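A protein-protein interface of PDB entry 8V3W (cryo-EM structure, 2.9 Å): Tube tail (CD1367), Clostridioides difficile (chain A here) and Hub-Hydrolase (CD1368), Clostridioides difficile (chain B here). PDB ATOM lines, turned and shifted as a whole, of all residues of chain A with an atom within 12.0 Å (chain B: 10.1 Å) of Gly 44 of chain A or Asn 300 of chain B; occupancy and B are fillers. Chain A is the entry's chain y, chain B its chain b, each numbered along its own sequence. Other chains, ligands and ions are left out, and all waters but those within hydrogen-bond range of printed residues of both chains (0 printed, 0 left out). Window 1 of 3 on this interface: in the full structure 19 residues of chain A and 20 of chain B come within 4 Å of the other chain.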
ATOM      1  N   LYS A  26      -3.043 -14.382  19.185  1.00  0.00           N
ATOM      2  CA  LYS A  26      -4.281 -13.811  18.678  1.00  0.00           C
ATOM      3  C   LYS A  26      -4.010 -13.027  17.404  1.00  0.00           C
ATOM      4  O   LYS A  26      -2.877 -12.646  17.110  1.00  0.00           O
ATOM      5  CB  LYS A  26      -4.950 -12.894  19.705  1.00  0.00           C
ATOM      6  CG  LYS A  26      -5.407 -13.599  20.960  1.00  0.00           C
ATOM      7  CD  LYS A  26      -6.176 -12.662  21.866  1.00  0.00           C
ATOM      8  CE  LYS A  26      -6.345 -13.258  23.252  1.00  0.00           C
ATOM      9  NZ  LYS A  26      -6.561 -14.728  23.197  1.00  0.00           N
ATOM     10  N   ALA A  27      -5.075 -12.798  16.646  1.00  0.00           N
ATOM     11  CA  ALA A  27      -5.051 -11.929  15.481  1.00  0.00           C
ATOM     12  C   ALA A  27      -6.165 -10.906  15.618  1.00  0.00           C
ATOM     13  O   ALA A  27      -7.248 -11.221  16.116  1.00  0.00           O
ATOM     14  CB  ALA A  27      -5.223 -12.718  14.185  1.00  0.00           C
ATOM     15  N   ALA A  28      -5.895  -9.680  15.185  1.00  0.00           N
ATOM     16  CA  ALA A  28      -6.879  -8.613  15.292  1.00  0.00           C
ATOM     17  C   ALA A  28      -7.853  -8.679  14.124  1.00  0.00           C
ATOM     18  O   ALA A  28      -7.442  -8.663  12.962  1.00  0.00           O
ATOM     19  CB  ALA A  28      -6.190  -7.253  15.331  1.00  0.00           C
ATOM     20  N   VAL A  29      -9.141  -8.749  14.433  1.00  0.00           N
ATOM     21  CA  VAL A  29     -10.191  -8.796  13.425  1.00  0.00           C
ATOM     22  C   VAL A  29     -11.076  -7.574  13.609  1.00  0.00           C
ATOM     23  O   VAL A  29     -11.741  -7.435  14.641  1.00  0.00           O
ATOM     24  CB  VAL A  29     -11.010 -10.091  13.513  1.00  0.00           C
ATOM     25  CG1 VAL A  29     -12.069 -10.107  12.450  1.00  0.00           C
ATOM     26  CG2 VAL A  29     -10.102 -11.291  13.359  1.00  0.00           C
ATOM     27  N   ASN A  30     -11.078  -6.691  12.616  1.00  0.00           N
ATOM     28  CA  ASN A  30     -11.918  -5.503  12.655  1.00  0.00           C
ATOM     29  C   ASN A  30     -13.351  -5.867  12.299  1.00  0.00           C
ATOM     30  O   ASN A  30     -13.594  -6.659  11.388  1.00  0.00           O
ATOM     31  CB  ASN A  30     -11.400  -4.444  11.685  1.00  0.00           C
ATOM     32  CG  ASN A  30      -9.900  -4.272  11.756  1.00  0.00           C
ATOM     33  OD1 ASN A  30      -9.303  -4.370  12.826  1.00  0.00           O
ATOM     34  ND2 ASN A  30      -9.281  -4.010  10.612  1.00  0.00           N
ATOM     35  N   SER A  31     -14.299  -5.277  13.017  1.00  0.00           N
ATOM     36  CA  SER A  31     -15.718  -5.519  12.798  1.00  0.00           C
ATOM     37  C   SER A  31     -16.378  -4.267  12.243  1.00  0.00           C
ATOM     38  O   SER A  31     -16.137  -3.162  12.737  1.00  0.00           O
ATOM     39  CB  SER A  31     -16.408  -5.946  14.092  1.00  0.00           C
ATOM     40  OG  SER A  31     -16.204  -7.323  14.341  1.00  0.00           O
ATOM     41  N   SER A  32     -17.197  -4.446  11.212  1.00  0.00           N
ATOM     42  CA  SER A  32     -18.005  -3.380  10.644  1.00  0.00           C
ATOM     43  C   SER A  32     -19.391  -3.949  10.381  1.00  0.00           C
ATOM     44  O   SER A  32     -19.729  -5.045  10.833  1.00  0.00           O
ATOM     45  CB  SER A  32     -17.368  -2.818   9.368  1.00  0.00           C
ATOM     46  OG  SER A  32     -16.019  -2.458   9.584  1.00  0.00           O
ATOM     47  N   ILE A  40     -19.768  -7.670   9.049  1.00  0.00           N
ATOM     48  CA  ILE A  40     -18.629  -8.105   8.249  1.00  0.00           C
ATOM     49  C   ILE A  40     -17.356  -7.915   9.063  1.00  0.00           C
ATOM     50  O   ILE A  40     -17.337  -7.210  10.073  1.00  0.00           O
ATOM     51  CB  ILE A  40     -18.517  -7.350   6.910  1.00  0.00           C
ATOM     52  CG1 ILE A  40     -18.279  -5.868   7.169  1.00  0.00           C
ATOM     53  CG2 ILE A  40     -19.755  -7.569   6.063  1.00  0.00           C
ATOM     54  CD1 ILE A  40     -17.993  -5.081   5.934  1.00  0.00           C
ATOM     55  N   ALA A  41     -16.281  -8.563   8.615  1.00  0.00           N
ATOM     56  CA  ALA A  41     -15.013  -8.538   9.332  1.00  0.00           C
ATOM     57  C   ALA A  41     -13.846  -8.475   8.358  1.00  0.00           C
ATOM     58  O   ALA A  41     -13.929  -8.975   7.234  1.00  0.00           O
ATOM     59  CB  ALA A  41     -14.860  -9.763  10.238  1.00  0.00           C
ATOM     60  N   THR A  42     -12.752  -7.860   8.804  1.00  0.00           N
ATOM     61  CA  THR A  42     -11.521  -7.782   8.028  1.00  0.00           C
ATOM     62  C   THR A  42     -10.329  -8.083   8.924  1.00  0.00           C
ATOM     63  O   THR A  42     -10.392  -7.945  10.145  1.00  0.00           O
ATOM     64  CB  THR A  42     -11.324  -6.405   7.376  1.00  0.00           C
ATOM     65  OG1 THR A  42     -11.317  -5.389   8.386  1.00  0.00           O
ATOM     66  CG2 THR A  42     -12.424  -6.116   6.374  1.00  0.00           C
ATOM     67  N   PHE A  43      -9.239  -8.507   8.290  1.00  0.00           N
ATOM     68  CA  PHE A  43      -7.995  -8.791   8.994  1.00  0.00           C
ATOM     69  C   PHE A  43      -7.336  -7.500   9.467  1.00  0.00           C
ATOM     70  O   PHE A  43      -7.312  -6.499   8.750  1.00  0.00           O
ATOM     71  CB  PHE A  43      -7.050  -9.561   8.074  1.00  0.00           C
ATOM     72  CG  PHE A  43      -5.753  -9.957   8.713  1.00  0.00           C
ATOM     73  CD1 PHE A  43      -5.733 -10.763   9.834  1.00  0.00           C
ATOM     74  CD2 PHE A  43      -4.550  -9.543   8.174  1.00  0.00           C
ATOM     75  CE1 PHE A  43      -4.543 -11.134  10.409  1.00  0.00           C
ATOM     76  CE2 PHE A  43      -3.353  -9.911   8.753  1.00  0.00           C
ATOM     77  CZ  PHE A  43      -3.351 -10.708   9.867  1.00  0.00           C
ATOM     78  N   GLY A  44      -6.791  -7.527  10.680  1.00  0.00           N
ATOM     79  CA  GLY A  44      -6.187  -6.338  11.246  1.00  0.00           C
ATOM     80  C   GLY A  44      -4.781  -6.501  11.787  1.00  0.00           C
ATOM     81  O   GLY A  44      -4.287  -5.623  12.496  1.00  0.00           O
ATOM     82  N   GLY A  45      -4.122  -7.604  11.463  1.00  0.00           N
ATOM     83  CA  GLY A  45      -2.757  -7.822  11.886  1.00  0.00           C
ATOM     84  C   GLY A  45      -2.663  -8.742  13.092  1.00  0.00           C
ATOM     85  O   GLY A  45      -3.620  -8.944  13.841  1.00  0.00           O
ATOM     86  N   VAL A  46      -1.481  -9.303  13.281  1.00  0.00           N
ATOM     87  CA  VAL A  46      -1.236 -10.296  14.320  1.00  0.00           C
ATOM     88  C   VAL A  46      -0.739  -9.597  15.577  1.00  0.00           C
ATOM     89  O   VAL A  46      -0.065  -8.565  15.515  1.00  0.00           O
ATOM     90  CB  VAL A  46      -0.235 -11.362  13.823  1.00  0.00           C
ATOM     91  CG1 VAL A  46       1.115 -10.740  13.529  1.00  0.00           C
ATOM     92  CG2 VAL A  46      -0.104 -12.500  14.815  1.00  0.00           C
ATOM     93  N   ALA A  47      -1.079 -10.158  16.733  1.00  0.00           N
ATOM     94  CA  ALA A  47      -0.668  -9.629  18.024  1.00  0.00           C
ATOM     95  C   ALA A  47       0.538 -10.388  18.568  1.00  0.00           C
ATOM     96  O   ALA A  47       0.899 -11.464  18.091  1.00  0.00           O
ATOM     97  CB  ALA A  47      -1.826  -9.695  19.018  1.00  0.00           C
ATOM     98  N   LEU A  48       1.157  -9.812  19.593  1.00  0.00           N
ATOM     99  CA  LEU A  48       2.324 -10.416  20.222  1.00  0.00           C
ATOM    100  C   LEU A  48       1.920 -11.566  21.135  1.00  0.00           C
ATOM    101  O   LEU A  48       0.915 -11.492  21.845  1.00  0.00           O
ATOM    102  CB  LEU A  48       3.095  -9.367  21.021  1.00  0.00           C
ATOM    103  CG  LEU A  48       3.539  -8.103  20.289  1.00  0.00           C
ATOM    104  CD1 LEU A  48       3.790  -6.988  21.278  1.00  0.00           C
ATOM    105  CD2 LEU A  48       4.778  -8.372  19.474  1.00  0.00           C
ATOM    106  N   LYS A 129       9.230  -7.065  19.456  1.00  0.00           N
ATOM    107  CA  LYS A 129       9.448  -6.950  18.020  1.00  0.00           C
ATOM    108  C   LYS A 129      10.137  -5.634  17.695  1.00  0.00           C
ATOM    109  O   LYS A 129       9.921  -4.620  18.362  1.00  0.00           O
ATOM    110  CB  LYS A 129       8.132  -7.041  17.241  1.00  0.00           C
ATOM    111  CG  LYS A 129       7.619  -8.453  17.046  1.00  0.00           C
ATOM    112  CD  LYS A 129       6.388  -8.482  16.160  1.00  0.00           C
ATOM    113  CE  LYS A 129       5.874  -9.900  15.974  1.00  0.00           C
ATOM    114  NZ  LYS A 129       4.597  -9.944  15.213  1.00  0.00           N
ATOM    115  N   ILE B   2      -0.508   1.873  -0.440  1.00  0.00           N
ATOM    116  CA  ILE B   2      -0.302   3.303  -0.255  1.00  0.00           C
ATOM    117  C   ILE B   2       1.154   3.526   0.124  1.00  0.00           C
ATOM    118  O   ILE B   2       1.701   2.797   0.957  1.00  0.00           O
ATOM    119  CB  ILE B   2      -1.249   3.889   0.810  1.00  0.00           C
ATOM    120  CG1 ILE B   2      -1.121   3.140   2.132  1.00  0.00           C
ATOM    121  CG2 ILE B   2      -2.681   3.816   0.335  1.00  0.00           C
ATOM    122  CD1 ILE B   2      -1.691   3.890   3.300  1.00  0.00           C
ATOM    123  N   VAL B  20       4.489   4.374   9.131  1.00  0.00           N
ATOM    124  CA  VAL B  20       3.247   5.120   9.283  1.00  0.00           C
ATOM    125  C   VAL B  20       2.241   4.334  10.110  1.00  0.00           C
ATOM    126  O   VAL B  20       2.106   3.113   9.977  1.00  0.00           O
ATOM    127  CB  VAL B  20       2.674   5.473   7.900  1.00  0.00           C
ATOM    128  CG1 VAL B  20       1.296   6.074   8.033  1.00  0.00           C
ATOM    129  CG2 VAL B  20       3.592   6.433   7.187  1.00  0.00           C
ATOM    130  N   ASP B  21       1.524   5.047  10.974  1.00  0.00           N
ATOM    131  CA  ASP B  21       0.530   4.478  11.872  1.00  0.00           C
ATOM    132  C   ASP B  21      -0.906   4.752  11.450  1.00  0.00           C
ATOM    133  O   ASP B  21      -1.775   3.917  11.696  1.00  0.00           O
ATOM    134  CB  ASP B  21       0.741   5.029  13.286  1.00  0.00           C
ATOM    135  CG  ASP B  21      -0.016   4.263  14.332  1.00  0.00           C
ATOM    136  OD1 ASP B  21      -1.205   4.567  14.548  1.00  0.00           O
ATOM    137  OD2 ASP B  21       0.584   3.372  14.962  1.00  0.00           O
ATOM    138  N   LYS B  22      -1.173   5.894  10.822  1.00  0.00           N
ATOM    139  CA  LYS B  22      -2.522   6.307  10.469  1.00  0.00           C
ATOM    140  C   LYS B  22      -2.425   7.400   9.416  1.00  0.00           C
ATOM    141  O   LYS B  22      -1.488   8.197   9.430  1.00  0.00           O
ATOM    142  CB  LYS B  22      -3.277   6.804  11.703  1.00  0.00           C
ATOM    143  CG  LYS B  22      -4.765   6.902  11.522  1.00  0.00           C
ATOM    144  CD  LYS B  22      -5.402   7.681  12.649  1.00  0.00           C
ATOM    145  CE  LYS B  22      -6.842   8.016  12.318  1.00  0.00           C
ATOM    146  NZ  LYS B  22      -6.958   8.539  10.932  1.00  0.00           N
ATOM    147  N   VAL B  23      -3.387   7.423   8.489  1.00  0.00           N
ATOM    148  CA  VAL B  23      -3.421   8.402   7.404  1.00  0.00           C
ATOM    149  C   VAL B  23      -4.838   8.942   7.258  1.00  0.00           C
ATOM    150  O   VAL B  23      -5.811   8.196   7.404  1.00  0.00           O
ATOM    151  CB  VAL B  23      -2.950   7.803   6.060  1.00  0.00           C
ATOM    152  CG1 VAL B  23      -2.814   8.888   5.013  1.00  0.00           C
ATOM    153  CG2 VAL B  23      -1.644   7.066   6.213  1.00  0.00           C
ATOM    154  N   ILE B  41       5.674   6.044  14.146  1.00  0.00           N
ATOM    155  CA  ILE B  41       6.067   5.450  15.418  1.00  0.00           C
ATOM    156  C   ILE B  41       7.512   5.819  15.709  1.00  0.00           C
ATOM    157  O   ILE B  41       8.410   5.531  14.913  1.00  0.00           O
ATOM    158  CB  ILE B  41       5.877   3.928  15.397  1.00  0.00           C
ATOM    159  CG1 ILE B  41       4.392   3.593  15.504  1.00  0.00           C
ATOM    160  CG2 ILE B  41       6.665   3.277  16.513  1.00  0.00           C
ATOM    161  CD1 ILE B  41       4.082   2.157  15.273  1.00  0.00           C
ATOM    162  N   GLU B  85       4.737   8.242  19.539  1.00  0.00           N
ATOM    163  CA  GLU B  85       4.194   8.704  18.268  1.00  0.00           C
ATOM    164  C   GLU B  85       4.548  10.168  18.054  1.00  0.00           C
ATOM    165  O   GLU B  85       4.684  10.934  19.010  1.00  0.00           O
ATOM    166  CB  GLU B  85       2.672   8.532  18.217  1.00  0.00           C
ATOM    167  CG  GLU B  85       2.196   7.118  17.974  1.00  0.00           C
ATOM    168  CD  GLU B  85       0.749   7.062  17.542  1.00  0.00           C
ATOM    169  OE1 GLU B  85       0.296   5.978  17.122  1.00  0.00           O
ATOM    170  OE2 GLU B  85       0.063   8.100  17.635  1.00  0.00           O
ATOM    171  N   THR B 297      -9.871   7.626   5.180  1.00  0.00           N
ATOM    172  CA  THR B 297      -9.025   7.210   6.290  1.00  0.00           C
ATOM    173  C   THR B 297      -8.520   5.794   6.070  1.00  0.00           C
ATOM    174  O   THR B 297      -9.271   4.917   5.645  1.00  0.00           O
ATOM    175  CB  THR B 297      -9.771   7.279   7.629  1.00  0.00           C
ATOM    176  OG1 THR B 297     -11.063   6.681   7.491  1.00  0.00           O
ATOM    177  CG2 THR B 297      -9.937   8.713   8.082  1.00  0.00           C
ATOM    178  N   TRP B 298      -7.237   5.584   6.353  1.00  0.00           N
ATOM    179  CA  TRP B 298      -6.624   4.263   6.364  1.00  0.00           C
ATOM    180  C   TRP B 298      -6.092   3.990   7.759  1.00  0.00           C
ATOM    181  O   TRP B 298      -5.299   4.775   8.286  1.00  0.00           O
ATOM    182  CB  TRP B 298      -5.488   4.160   5.348  1.00  0.00           C
ATOM    183  CG  TRP B 298      -5.919   4.235   3.925  1.00  0.00           C
ATOM    184  CD1 TRP B 298      -6.222   3.192   3.108  1.00  0.00           C
ATOM    185  CD2 TRP B 298      -6.085   5.419   3.143  1.00  0.00           C
ATOM    186  NE1 TRP B 298      -6.571   3.650   1.865  1.00  0.00           N
ATOM    187  CE2 TRP B 298      -6.494   5.016   1.861  1.00  0.00           C
ATOM    188  CE3 TRP B 298      -5.924   6.779   3.402  1.00  0.00           C
ATOM    189  CZ2 TRP B 298      -6.745   5.922   0.844  1.00  0.00           C
ATOM    190  CZ3 TRP B 298      -6.176   7.675   2.391  1.00  0.00           C
ATOM    191  CH2 TRP B 298      -6.583   7.246   1.129  1.00  0.00           C
ATOM    192  N   GLN B 299      -6.516   2.877   8.350  1.00  0.00           N
ATOM    193  CA  GLN B 299      -6.086   2.522   9.696  1.00  0.00           C
ATOM    194  C   GLN B 299      -6.403   1.068  10.007  1.00  0.00           C
ATOM    195  O   GLN B 299      -7.522   0.608   9.763  1.00  0.00           O
ATOM    196  CB  GLN B 299      -6.750   3.429  10.729  1.00  0.00           C
ATOM    197  CG  GLN B 299      -6.235   3.229  12.137  1.00  0.00           C
ATOM    198  CD  GLN B 299      -6.976   4.070  13.153  1.00  0.00           C
ATOM    199  OE1 GLN B 299      -7.946   4.749  12.822  1.00  0.00           O
ATOM    200  NE2 GLN B 299      -6.520   4.034  14.397  1.00  0.00           N
ATOM    201  N   ASN B 300      -5.425   0.342  10.546  1.00  0.00           N
ATOM    202  CA  ASN B 300      -5.595  -1.052  10.956  1.00  0.00           C
ATOM    203  C   ASN B 300      -6.015  -1.943   9.793  1.00  0.00           C
ATOM    204  O   ASN B 300      -6.761  -2.905   9.975  1.00  0.00           O
ATOM    205  CB  ASN B 300      -6.602  -1.176  12.101  1.00  0.00           C
ATOM    206  CG  ASN B 300      -6.004  -0.826  13.438  1.00  0.00           C
ATOM    207  OD1 ASN B 300      -4.795  -0.936  13.632  1.00  0.00           O
ATOM    208  ND2 ASN B 300      -6.845  -0.401  14.370  1.00  0.00           N
ATOM    209  N   GLY B 301      -5.548  -1.634   8.589  1.00  0.00           N
ATOM    210  CA  GLY B 301      -5.882  -2.457   7.448  1.00  0.00           C
ATOM    211  C   GLY B 301      -7.301  -2.333   6.942  1.00  0.00           C
ATOM    212  O   GLY B 301      -7.794  -3.260   6.300  1.00  0.00           O
ATOM    213  N   GLU B 302      -7.980  -1.219   7.212  1.00  0.00           N
ATOM    214  CA  GLU B 302      -9.307  -0.982   6.665  1.00  0.00           C
ATOM    215  C   GLU B 302      -9.406   0.451   6.165  1.00  0.00           C
ATOM    216  O   GLU B 302      -8.718   1.345   6.659  1.00  0.00           O
ATOM    217  CB  GLU B 302     -10.401  -1.274   7.693  1.00  0.00           C
ATOM    218  CG  GLU B 302     -10.467  -0.308   8.843  1.00  0.00           C
ATOM    219  CD  GLU B 302     -11.745  -0.465   9.635  1.00  0.00           C
ATOM    220  OE1 GLU B 302     -12.577  -1.314   9.251  1.00  0.00           O
ATOM    221  OE2 GLU B 302     -11.920   0.254  10.640  1.00  0.00           O
ATOM    222  N   TYR B 303     -10.278   0.658   5.179  1.00  0.00           N
ATOM    223  CA  TYR B 303     -10.377   1.922   4.458  1.00  0.00           C
ATOM    224  C   TYR B 303     -11.845   2.295   4.310  1.00  0.00           C
ATOM    225  O   TYR B 303     -12.630   1.515   3.768  1.00  0.00           O
ATOM    226  CB  TYR B 303      -9.695   1.797   3.091  1.00  0.00           C
ATOM    227  CG  TYR B 303      -9.947   2.924   2.124  1.00  0.00           C
ATOM    228  CD1 TYR B 303      -9.874   4.244   2.530  1.00  0.00           C
ATOM    229  CD2 TYR B 303     -10.234   2.665   0.795  1.00  0.00           C
ATOM    230  CE1 TYR B 303     -10.090   5.268   1.645  1.00  0.00           C
ATOM    231  CE2 TYR B 303     -10.456   3.687  -0.098  1.00  0.00           C
ATOM    232  CZ  TYR B 303     -10.384   4.987   0.335  1.00  0.00           C
ATOM    233  OH  TYR B 303     -10.602   6.016  -0.545  1.00  0.00           O
ATOM    234  N   GLN B 304     -12.213   3.489   4.780  1.00  0.00           N
ATOM    235  CA  GLN B 304     -13.597   3.946   4.759  1.00  0.00           C
ATOM    236  C   GLN B 304     -13.654   5.397   4.299  1.00  0.00           C
ATOM    237  O   GLN B 304     -12.676   6.135   4.399  1.00  0.00           O
ATOM    238  CB  GLN B 304     -14.254   3.809   6.134  1.00  0.00           C
ATOM    239  CG  GLN B 304     -14.520   2.379   6.553  1.00  0.00           C
ATOM    240  CD  GLN B 304     -14.864   2.260   8.019  1.00  0.00           C
ATOM    241  OE1 GLN B 304     -15.049   3.260   8.703  1.00  0.00           O
ATOM    242  NE2 GLN B 304     -14.955   1.034   8.508  1.00  0.00           N
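The backbone carbonyl oxygen of Asn 300 of chain B sits at hydrogen-bond distance from the side-chain amide nitrogen of Asn 30 of chain A, at 2.8 Å.
The backbone carbonyl oxygen (O) of Ile 40 of chain A sits at hydrogen-bond distance from the backbone NH (N) of Ser 32 of chain A (3.0 Å). N of Gly 44 of chain A lies within hydrogen-bond range of O of Ala 28 of chain A (2.6 Å). N of Asn 30 of chain A sits at hydrogen-bond distance from O of Thr 42 of chain A. The backbone NH of Thr 297 of chain B sits at hydrogen-bond distance from the backbone carbonyl oxygen of Gln 304 of chain B. OE1 of Glu 302 of chain B sits at hydrogen-bond distance from NE2 of Gln 304 of chain B, 3.4 Å away.
Glu 302 of chain B touches Ser 32 of chain A (OE1 to OG, 3.6 Å). OG of Ser 32 of chain A touches NE2 of Gln 304 of chain B (3.8 Å). Asn 300 of chain B touches Phe 43 of chain A. Gly 44 of chain A touches Asn 300 of chain B (CA to O, 3.7 Å).
Ala 28 of chain A touches none of the printed residues of chain B. Printed residues of chain B within 4 Å of Asn 30 of chain A: Asn 300. Of the printed residues of chain B, Ser 32 of chain A touches Glu 302 and Gln 304. Gly 44 of chain A touches just one residue of chain B: Asn 300 (3.7 Å). No residue of chain B comes within 4 Å of Gly 45 of chain A. No residue of chain A comes within 4 Å of Gln 299 of chain B. Asn 300 of chain B touches just these residues of chain A: Asn 30, Phe 43 and Gly 44. No residue of chain A comes within 4 Å of Gly 301 of chain B. Printed residues of chain A within 4 Å of Gln 304 of chain B: Ser 32. The nearest residue of chain B that does not touch Gly 44 of chain A is Gly 301 of chain B (5.4 Å). The nearest residue of chain A that does not touch Asn 300 of chain B is Thr 42 of chain A (5.4 Å).
Of the 15 printed residues of chain B, 3 touch a printed residue of chain A. Among the printed residues, 5 pairs touch across the chains.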
